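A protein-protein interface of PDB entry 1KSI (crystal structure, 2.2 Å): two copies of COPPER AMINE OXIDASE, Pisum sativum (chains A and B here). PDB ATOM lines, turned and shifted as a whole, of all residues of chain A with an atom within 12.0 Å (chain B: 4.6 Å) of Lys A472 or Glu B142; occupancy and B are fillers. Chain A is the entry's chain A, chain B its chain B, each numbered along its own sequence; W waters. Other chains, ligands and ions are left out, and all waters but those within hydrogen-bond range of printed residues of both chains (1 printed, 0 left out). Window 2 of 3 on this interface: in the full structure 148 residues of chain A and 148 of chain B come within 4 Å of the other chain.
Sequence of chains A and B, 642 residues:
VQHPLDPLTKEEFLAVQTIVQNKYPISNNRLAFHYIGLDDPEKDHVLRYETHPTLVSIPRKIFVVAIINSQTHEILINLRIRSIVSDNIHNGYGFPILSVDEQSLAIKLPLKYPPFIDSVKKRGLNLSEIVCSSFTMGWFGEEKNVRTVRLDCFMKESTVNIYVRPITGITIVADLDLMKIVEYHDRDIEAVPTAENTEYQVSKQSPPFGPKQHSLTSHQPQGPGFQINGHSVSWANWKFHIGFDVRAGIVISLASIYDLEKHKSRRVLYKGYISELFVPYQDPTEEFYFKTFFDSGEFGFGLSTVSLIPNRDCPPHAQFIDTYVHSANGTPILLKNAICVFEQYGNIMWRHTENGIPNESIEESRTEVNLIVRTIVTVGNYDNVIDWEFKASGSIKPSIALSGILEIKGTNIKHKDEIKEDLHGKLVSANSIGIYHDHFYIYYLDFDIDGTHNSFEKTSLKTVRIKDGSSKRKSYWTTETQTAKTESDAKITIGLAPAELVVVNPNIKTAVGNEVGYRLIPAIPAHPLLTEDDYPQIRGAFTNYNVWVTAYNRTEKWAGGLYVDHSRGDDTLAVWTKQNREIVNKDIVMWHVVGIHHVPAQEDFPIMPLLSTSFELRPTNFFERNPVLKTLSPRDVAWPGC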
ATOM      1  N   VAL A 464      -7.100  16.911   2.527  1.00  0.00           N
ATOM      2  CA  VAL A 464      -7.581  18.097   3.236  1.00  0.00           C
ATOM      3  C   VAL A 464      -8.766  18.642   2.430  1.00  0.00           C
ATOM      4  O   VAL A 464      -8.677  18.846   1.224  1.00  0.00           O
ATOM      5  CB  VAL A 464      -6.480  19.164   3.372  1.00  0.00           C
ATOM      6  CG1 VAL A 464      -6.982  20.368   4.140  1.00  0.00           C
ATOM      7  CG2 VAL A 464      -5.221  18.574   4.020  1.00  0.00           C
ATOM      8  N   ARG A 465      -9.892  18.800   3.069  1.00  0.00           N
ATOM      9  CA  ARG A 465     -11.098  19.389   2.502  1.00  0.00           C
ATOM     10  C   ARG A 465     -11.173  20.882   2.866  1.00  0.00           C
ATOM     11  O   ARG A 465     -11.184  21.148   4.062  1.00  0.00           O
ATOM     12  CB  ARG A 465     -12.367  18.682   3.002  1.00  0.00           C
ATOM     13  CG  ARG A 465     -13.571  19.322   2.313  1.00  0.00           C
ATOM     14  CD  ARG A 465     -14.864  18.610   2.620  1.00  0.00           C
ATOM     15  NE  ARG A 465     -15.288  17.674   1.591  1.00  0.00           N
ATOM     16  CZ  ARG A 465     -15.655  17.963   0.335  1.00  0.00           C
ATOM     17  NH1 ARG A 465     -15.651  19.219  -0.105  1.00  0.00           N
ATOM     18  NH2 ARG A 465     -16.015  16.931  -0.444  1.00  0.00           N
ATOM     19  N   ILE A 466     -11.164  21.809   1.928  1.00  0.00           N
ATOM     20  CA  ILE A 466     -11.241  23.250   2.152  1.00  0.00           C
ATOM     21  C   ILE A 466     -12.686  23.609   2.520  1.00  0.00           C
ATOM     22  O   ILE A 466     -13.571  23.437   1.668  1.00  0.00           O
ATOM     23  CB  ILE A 466     -10.831  24.051   0.915  1.00  0.00           C
ATOM     24  CG1 ILE A 466      -9.321  23.937   0.651  1.00  0.00           C
ATOM     25  CG2 ILE A 466     -11.244  25.525   0.932  1.00  0.00           C
ATOM     26  CD1 ILE A 466      -8.957  23.900  -0.818  1.00  0.00           C
ATOM     27  N   LYS A 467     -12.869  24.059   3.775  1.00  0.00           N
ATOM     28  CA  LYS A 467     -14.200  24.336   4.301  1.00  0.00           C
ATOM     29  C   LYS A 467     -14.591  25.811   4.188  1.00  0.00           C
ATOM     30  O   LYS A 467     -15.747  26.190   3.942  1.00  0.00           O
ATOM     31  N   ASP A 468     -13.592  26.677   4.337  1.00  0.00           N
ATOM     32  CA  ASP A 468     -13.783  28.116   4.322  1.00  0.00           C
ATOM     33  C   ASP A 468     -13.885  28.828   2.985  1.00  0.00           C
ATOM     34  O   ASP A 468     -13.643  30.068   2.957  1.00  0.00           O
ATOM     35  CB  ASP A 468     -12.630  28.713   5.175  1.00  0.00           C
ATOM     36  CG  ASP A 468     -11.282  28.408   4.544  1.00  0.00           C
ATOM     37  OD1 ASP A 468     -11.247  27.609   3.577  1.00  0.00           O
ATOM     38  OD2 ASP A 468     -10.262  28.977   5.009  1.00  0.00           O
ATOM     39  N   GLY A 469     -14.255  28.173   1.883  1.00  0.00           N
ATOM     40  CA  GLY A 469     -14.345  28.897   0.620  1.00  0.00           C
ATOM     41  C   GLY A 469     -13.163  29.817   0.330  1.00  0.00           C
ATOM     42  O   GLY A 469     -13.277  30.823  -0.398  1.00  0.00           O
ATOM     43  N   SER A 470     -11.983  29.530   0.866  1.00  0.00           N
ATOM     44  CA  SER A 470     -10.788  30.300   0.549  1.00  0.00           C
ATOM     45  C   SER A 470     -10.081  29.789  -0.703  1.00  0.00           C
ATOM     46  O   SER A 470      -8.972  30.249  -1.012  1.00  0.00           O
ATOM     47  CB  SER A 470      -9.805  30.152   1.721  1.00  0.00           C
ATOM     48  OG  SER A 470      -9.643  28.732   1.964  1.00  0.00           O
ATOM     49  N   SER A 471     -10.633  28.813  -1.429  1.00  0.00           N
ATOM     50  CA  SER A 471     -10.059  28.354  -2.689  1.00  0.00           C
ATOM     51  C   SER A 471     -11.196  27.980  -3.642  1.00  0.00           C
ATOM     52  O   SER A 471     -12.291  27.739  -3.135  1.00  0.00           O
ATOM     53  CB  SER A 471      -9.153  27.125  -2.489  1.00  0.00           C
ATOM     54  OG  SER A 471      -8.477  26.778  -3.685  1.00  0.00           O
ATOM     55  N   LYS A 472     -10.961  27.969  -4.953  1.00  0.00           N
ATOM     56  CA  LYS A 472     -11.938  27.410  -5.895  1.00  0.00           C
ATOM     57  C   LYS A 472     -11.966  25.879  -5.753  1.00  0.00           C
ATOM     58  O   LYS A 472     -12.968  25.209  -6.004  1.00  0.00           O
ATOM     59  CB  LYS A 472     -11.614  27.830  -7.332  1.00  0.00           C
ATOM     60  CG  LYS A 472     -11.936  29.312  -7.586  1.00  0.00           C
ATOM     61  CD  LYS A 472     -11.989  29.738  -9.038  1.00  0.00           C
ATOM     62  CE  LYS A 472     -13.267  30.483  -9.466  1.00  0.00           C
ATOM     63  NZ  LYS A 472     -13.640  30.205 -10.918  1.00  0.00           N
ATOM     64  N   ARG A 473     -10.828  25.305  -5.331  1.00  0.00           N
ATOM     65  CA  ARG A 473     -10.662  23.871  -5.071  1.00  0.00           C
ATOM     66  C   ARG A 473     -11.393  23.425  -3.821  1.00  0.00           C
ATOM     67  O   ARG A 473     -11.318  24.149  -2.811  1.00  0.00           O
ATOM     68  CB  ARG A 473      -9.154  23.560  -4.885  1.00  0.00           C
ATOM     69  CG  ARG A 473      -8.457  23.550  -6.239  1.00  0.00           C
ATOM     70  CD  ARG A 473      -8.773  22.223  -6.985  1.00  0.00           C
ATOM     71  NE  ARG A 473      -7.938  21.162  -6.386  1.00  0.00           N
ATOM     72  CZ  ARG A 473      -6.670  20.825  -6.568  1.00  0.00           C
ATOM     73  NH1 ARG A 473      -5.780  21.339  -7.403  1.00  0.00           N
ATOM     74  NH2 ARG A 473      -6.275  19.847  -5.721  1.00  0.00           N
ATOM     75  N   LYS A 474     -12.084  22.289  -3.829  1.00  0.00           N
ATOM     76  CA  LYS A 474     -12.681  21.762  -2.599  1.00  0.00           C
ATOM     77  C   LYS A 474     -11.734  20.936  -1.729  1.00  0.00           C
ATOM     78  O   LYS A 474     -12.049  20.599  -0.570  1.00  0.00           O
ATOM     79  CB  LYS A 474     -13.870  20.859  -2.967  1.00  0.00           C
ATOM     80  CG  LYS A 474     -14.893  21.558  -3.847  1.00  0.00           C
ATOM     81  CD  LYS A 474     -16.245  20.860  -3.740  1.00  0.00           C
ATOM     82  CE  LYS A 474     -17.330  21.659  -4.478  1.00  0.00           C
ATOM     83  NZ  LYS A 474     -18.300  20.767  -5.227  1.00  0.00           N
ATOM     84  N   SER A 475     -10.574  20.567  -2.258  1.00  0.00           N
ATOM     85  CA  SER A 475      -9.709  19.609  -1.573  1.00  0.00           C
ATOM     86  C   SER A 475      -8.325  19.565  -2.222  1.00  0.00           C
ATOM     87  O   SER A 475      -8.061  19.994  -3.365  1.00  0.00           O
ATOM     88  CB  SER A 475     -10.312  18.191  -1.608  1.00  0.00           C
ATOM     89  OG  SER A 475     -10.250  17.643  -2.925  1.00  0.00           O
ATOM     90  N   TYR A 476      -7.385  19.097  -1.393  1.00  0.00           N
ATOM     91  CA  TYR A 476      -6.031  18.778  -1.876  1.00  0.00           C
ATOM     92  C   TYR A 476      -5.438  17.745  -0.888  1.00  0.00           C
ATOM     93  O   TYR A 476      -6.075  17.510   0.167  1.00  0.00           O
ATOM     94  CB  TYR A 476      -5.151  19.999  -2.034  1.00  0.00           C
ATOM     95  CG  TYR A 476      -5.028  20.709  -0.708  1.00  0.00           C
ATOM     96  CD1 TYR A 476      -6.052  21.457  -0.173  1.00  0.00           C
ATOM     97  CD2 TYR A 476      -3.844  20.536   0.007  1.00  0.00           C
ATOM     98  CE1 TYR A 476      -5.894  22.030   1.072  1.00  0.00           C
ATOM     99  CE2 TYR A 476      -3.686  21.134   1.255  1.00  0.00           C
ATOM    100  CZ  TYR A 476      -4.723  21.889   1.792  1.00  0.00           C
ATOM    101  OH  TYR A 476      -4.547  22.476   3.020  1.00  0.00           O
ATOM    102  N   GLY B 138      -9.308  24.291 -16.829  1.00  0.00           N
ATOM    103  CA  GLY B 138     -10.363  23.396 -16.333  1.00  0.00           C
ATOM    104  C   GLY B 138     -11.618  24.218 -16.083  1.00  0.00           C
ATOM    105  O   GLY B 138     -11.938  25.150 -16.839  1.00  0.00           O
ATOM    106  N   TRP B 139     -12.333  23.821 -15.039  1.00  0.00           N
ATOM    107  CA  TRP B 139     -13.628  24.420 -14.761  1.00  0.00           C
ATOM    108  C   TRP B 139     -13.942  24.307 -13.279  1.00  0.00           C
ATOM    109  O   TRP B 139     -13.692  23.271 -12.661  1.00  0.00           O
ATOM    110  CB  TRP B 139     -14.701  23.818 -15.663  1.00  0.00           C
ATOM    111  CG  TRP B 139     -16.066  24.261 -15.211  1.00  0.00           C
ATOM    112  CD1 TRP B 139     -16.711  25.450 -15.421  1.00  0.00           C
ATOM    113  CD2 TRP B 139     -16.945  23.464 -14.416  1.00  0.00           C
ATOM    114  NE1 TRP B 139     -17.927  25.425 -14.801  1.00  0.00           N
ATOM    115  CE2 TRP B 139     -18.098  24.222 -14.189  1.00  0.00           C
ATOM    116  CE3 TRP B 139     -16.852  22.154 -13.913  1.00  0.00           C
ATOM    117  CZ2 TRP B 139     -19.165  23.705 -13.479  1.00  0.00           C
ATOM    118  CZ3 TRP B 139     -17.907  21.638 -13.198  1.00  0.00           C
ATOM    119  CH2 TRP B 139     -19.051  22.427 -12.986  1.00  0.00           C
ATOM    120  N   PHE B 140     -14.475  25.394 -12.706  1.00  0.00           N
ATOM    121  CA  PHE B 140     -14.686  25.374 -11.257  1.00  0.00           C
ATOM    122  C   PHE B 140     -16.077  25.803 -10.866  1.00  0.00           C
ATOM    123  O   PHE B 140     -16.188  26.491  -9.861  1.00  0.00           O
ATOM    124  CB  PHE B 140     -13.581  26.199 -10.600  1.00  0.00           C
ATOM    125  CG  PHE B 140     -12.269  25.443 -10.536  1.00  0.00           C
ATOM    126  CD1 PHE B 140     -11.380  25.511 -11.602  1.00  0.00           C
ATOM    127  CD2 PHE B 140     -11.937  24.668  -9.427  1.00  0.00           C
ATOM    128  CE1 PHE B 140     -10.187  24.832 -11.563  1.00  0.00           C
ATOM    129  CE2 PHE B 140     -10.730  23.988  -9.393  1.00  0.00           C
ATOM    130  CZ  PHE B 140      -9.860  24.073 -10.455  1.00  0.00           C
ATOM    131  N   GLY B 141     -17.112  25.428 -11.621  1.00  0.00           N
ATOM    132  CA  GLY B 141     -18.462  25.804 -11.162  1.00  0.00           C
ATOM    133  C   GLY B 141     -19.027  27.003 -11.917  1.00  0.00           C
ATOM    134  O   GLY B 141     -20.228  27.039 -12.168  1.00  0.00           O
ATOM    135  N   GLU B 142     -18.192  27.958 -12.279  1.00  0.00           N
ATOM    136  CA  GLU B 142     -18.562  29.135 -13.022  1.00  0.00           C
ATOM    137  C   GLU B 142     -19.413  28.834 -14.253  1.00  0.00           C
ATOM    138  O   GLU B 142     -19.401  27.731 -14.795  1.00  0.00           O
ATOM    139  CB  GLU B 142     -17.301  29.898 -13.433  1.00  0.00           C
ATOM    140  CG  GLU B 142     -16.554  29.270 -14.605  1.00  0.00           C
ATOM    141  CD  GLU B 142     -15.476  28.288 -14.145  1.00  0.00           C
ATOM    142  OE1 GLU B 142     -15.250  28.124 -12.932  1.00  0.00           O
ATOM    143  OE2 GLU B 142     -14.839  27.709 -15.051  1.00  0.00           O
ATOM    144  N   GLU B 143     -20.158  29.849 -14.716  1.00  0.00           N
ATOM    145  CA  GLU B 143     -21.087  29.767 -15.826  1.00  0.00           C
ATOM    146  C   GLU B 143     -20.444  29.970 -17.184  1.00  0.00           C
ATOM    147  O   GLU B 143     -20.841  29.320 -18.171  1.00  0.00           O
ATOM    148  N   LYS B 144     -19.453  30.854 -17.223  1.00  0.00           N
ATOM    149  CA  LYS B 144     -18.722  31.125 -18.448  1.00  0.00           C
ATOM    150  C   LYS B 144     -18.340  29.846 -19.185  1.00  0.00           C
ATOM    151  O   LYS B 144     -18.123  28.807 -18.577  1.00  0.00           O
ATOM    152  CB  LYS B 144     -17.380  31.787 -18.197  1.00  0.00           C
ATOM    153  CG  LYS B 144     -17.356  32.871 -17.143  1.00  0.00           C
ATOM    154  CD  LYS B 144     -16.333  33.888 -17.684  1.00  0.00           C
ATOM    155  CE  LYS B 144     -15.678  34.692 -16.562  1.00  0.00           C
ATOM    156  NZ  LYS B 144     -14.397  35.328 -17.043  1.00  0.00           N
ATOM    157  N   TYR B 289      -4.179  26.380  -7.921  1.00  0.00           N
ATOM    158  CA  TYR B 289      -5.414  25.607  -7.843  1.00  0.00           C
ATOM    159  C   TYR B 289      -5.919  24.995  -9.142  1.00  0.00           C
ATOM    160  O   TYR B 289      -6.604  23.958  -9.111  1.00  0.00           O
ATOM    161  CB  TYR B 289      -6.508  26.506  -7.185  1.00  0.00           C
ATOM    162  CG  TYR B 289      -7.150  27.456  -8.204  1.00  0.00           C
ATOM    163  CD1 TYR B 289      -6.552  28.654  -8.539  1.00  0.00           C
ATOM    164  CD2 TYR B 289      -8.322  27.071  -8.850  1.00  0.00           C
ATOM    165  CE1 TYR B 289      -7.110  29.467  -9.512  1.00  0.00           C
ATOM    166  CE2 TYR B 289      -8.887  27.857  -9.842  1.00  0.00           C
ATOM    167  CZ  TYR B 289      -8.274  29.064 -10.135  1.00  0.00           C
ATOM    168  OH  TYR B 289      -8.840  29.869 -11.087  1.00  0.00           O
ATOM    169  N   TYR B 535     -13.948  19.639  -8.104  1.00  0.00           N
ATOM    170  CA  TYR B 535     -14.070  19.778  -9.533  1.00  0.00           C
ATOM    171  C   TYR B 535     -13.153  18.961 -10.429  1.00  0.00           C
ATOM    172  O   TYR B 535     -13.704  18.347 -11.365  1.00  0.00           O
ATOM    173  CB  TYR B 535     -13.965  21.274 -10.001  1.00  0.00           C
ATOM    174  CG  TYR B 535     -15.070  22.037  -9.302  1.00  0.00           C
ATOM    175  CD1 TYR B 535     -16.375  21.864  -9.727  1.00  0.00           C
ATOM    176  CD2 TYR B 535     -14.783  22.836  -8.208  1.00  0.00           C
ATOM    177  CE1 TYR B 535     -17.395  22.520  -9.068  1.00  0.00           C
ATOM    178  CE2 TYR B 535     -15.800  23.488  -7.550  1.00  0.00           C
ATOM    179  CZ  TYR B 535     -17.100  23.328  -7.986  1.00  0.00           C
ATOM    180  OH  TYR B 535     -18.130  23.985  -7.333  1.00  0.00           O
ATOM    181  N   ARG B 568     -17.111  19.729 -18.018  1.00  0.00           N
ATOM    182  CA  ARG B 568     -17.773  19.782 -16.711  1.00  0.00           C
ATOM    183  C   ARG B 568     -17.990  18.388 -16.148  1.00  0.00           C
ATOM    184  O   ARG B 568     -18.699  18.202 -15.157  1.00  0.00           O
ATOM    185  CB  ARG B 568     -19.062  20.631 -16.936  1.00  0.00           C
ATOM    186  CG  ARG B 568     -18.675  22.036 -17.371  1.00  0.00           C
ATOM    187  CD  ARG B 568     -19.758  23.080 -17.395  1.00  0.00           C
ATOM    188  NE  ARG B 568     -19.246  24.414 -17.768  1.00  0.00           N
ATOM    189  CZ  ARG B 568     -19.991  25.524 -17.646  1.00  0.00           C
ATOM    190  NH1 ARG B 568     -21.251  25.511 -17.177  1.00  0.00           N
ATOM    191  NH2 ARG B 568     -19.471  26.693 -17.987  1.00  0.00           N
HETATM  192  O   HOH W   1     -11.040  29.096 -12.554  1.00  0.00           O
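The guanidinium group of Arg A473 is in hydrogen-bond range of the backbone carbonyl oxygen of Tyr B289, 3.2 Å away.
The side-chain amino group (NZ) of Lys A472 lies within salt-bridge range of the side-chain carboxylate (OE1) of Glu B142 (3.3 Å).
O of Lys A474 lies within hydrogen-bond range of N of Ile A466 (2.9 Å).
The backbone carbonyl oxygen (O) of Ser A475 is in hydrogen-bond range of the guanidinium group (NH2) of Arg A473, 3.0 Å away.
OG of Ser A471 lies close to N of Arg A473 (3.2 Å).
The indole nitrogen of Trp B139 sits at hydrogen-bond distance from the backbone carbonyl oxygen of Glu B142 (2.7 Å).
The backbone carbonyl oxygen (O) of Glu B142 is in hydrogen-bond range of the guanidinium group (NH2) of Arg B568, 3.4 Å away.
The backbone NH (N) of Phe B140 sits at hydrogen-bond distance from the side-chain carboxylate (OE1) of Glu B142 (2.8 Å).
Among the printed residues, merely in contact across the chains: Arg A473 with Phe B140 (3.6 Å), Lys A472 with Phe B140 (3.6 Å), Lys A472 with Tyr B535 (3.7 Å), Lys A472 with Tyr B289 (3.7 Å) and Lys A474 with Tyr B535 (3.8 Å).
Ser A470 touches none of the printed residues of chain B.
Lys A472 touches just these residues of chain B: Phe B140 (3.6 Å), Glu B142 (3.3 Å), Tyr B289 (3.7 Å) and Tyr B535 (3.7 Å).
Of the printed residues of chain B, Arg A473 touches Phe B140 (3.6 Å) and Tyr B289 (3.2 Å).
Printed residues of chain B within 4 Å of Lys A474: Tyr B535.
No residue of chain A comes within 4 Å of Trp B139.
Of chain A, only Lys A472 and Arg A473 come within 4 Å of Phe B140.
Printed residues of chain A within 4 Å of Glu B142: Lys A472.
No residue of chain A comes within 4 Å of Lys B144.
Printed residues of chain A within 4 Å of Tyr B535: Lys A472 and Lys A474.
The nearest printed residue of chain B that does not touch Lys A472 is Gly B141 (5.9 Å).
The nearest residue of chain A that does not touch Glu B142 is Arg A473 (9.2 Å).
Hydrophobic or aromatic side chains of chain B that line the printed part of chain A: Phe B140, Tyr B289 and Tyr B535.
Among the printed residues, Asp or Glu carboxylates within 4 Å of a Lys or Arg side-chain nitrogen of the other chain: Lys A472 with Glu B142 (3.3 Å).
No position is printed for both chains.
Water W1 lies within hydrogen-bond range of OH of Tyr B289 (2.8 Å) and NZ of Lys A472 (3.3 Å).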
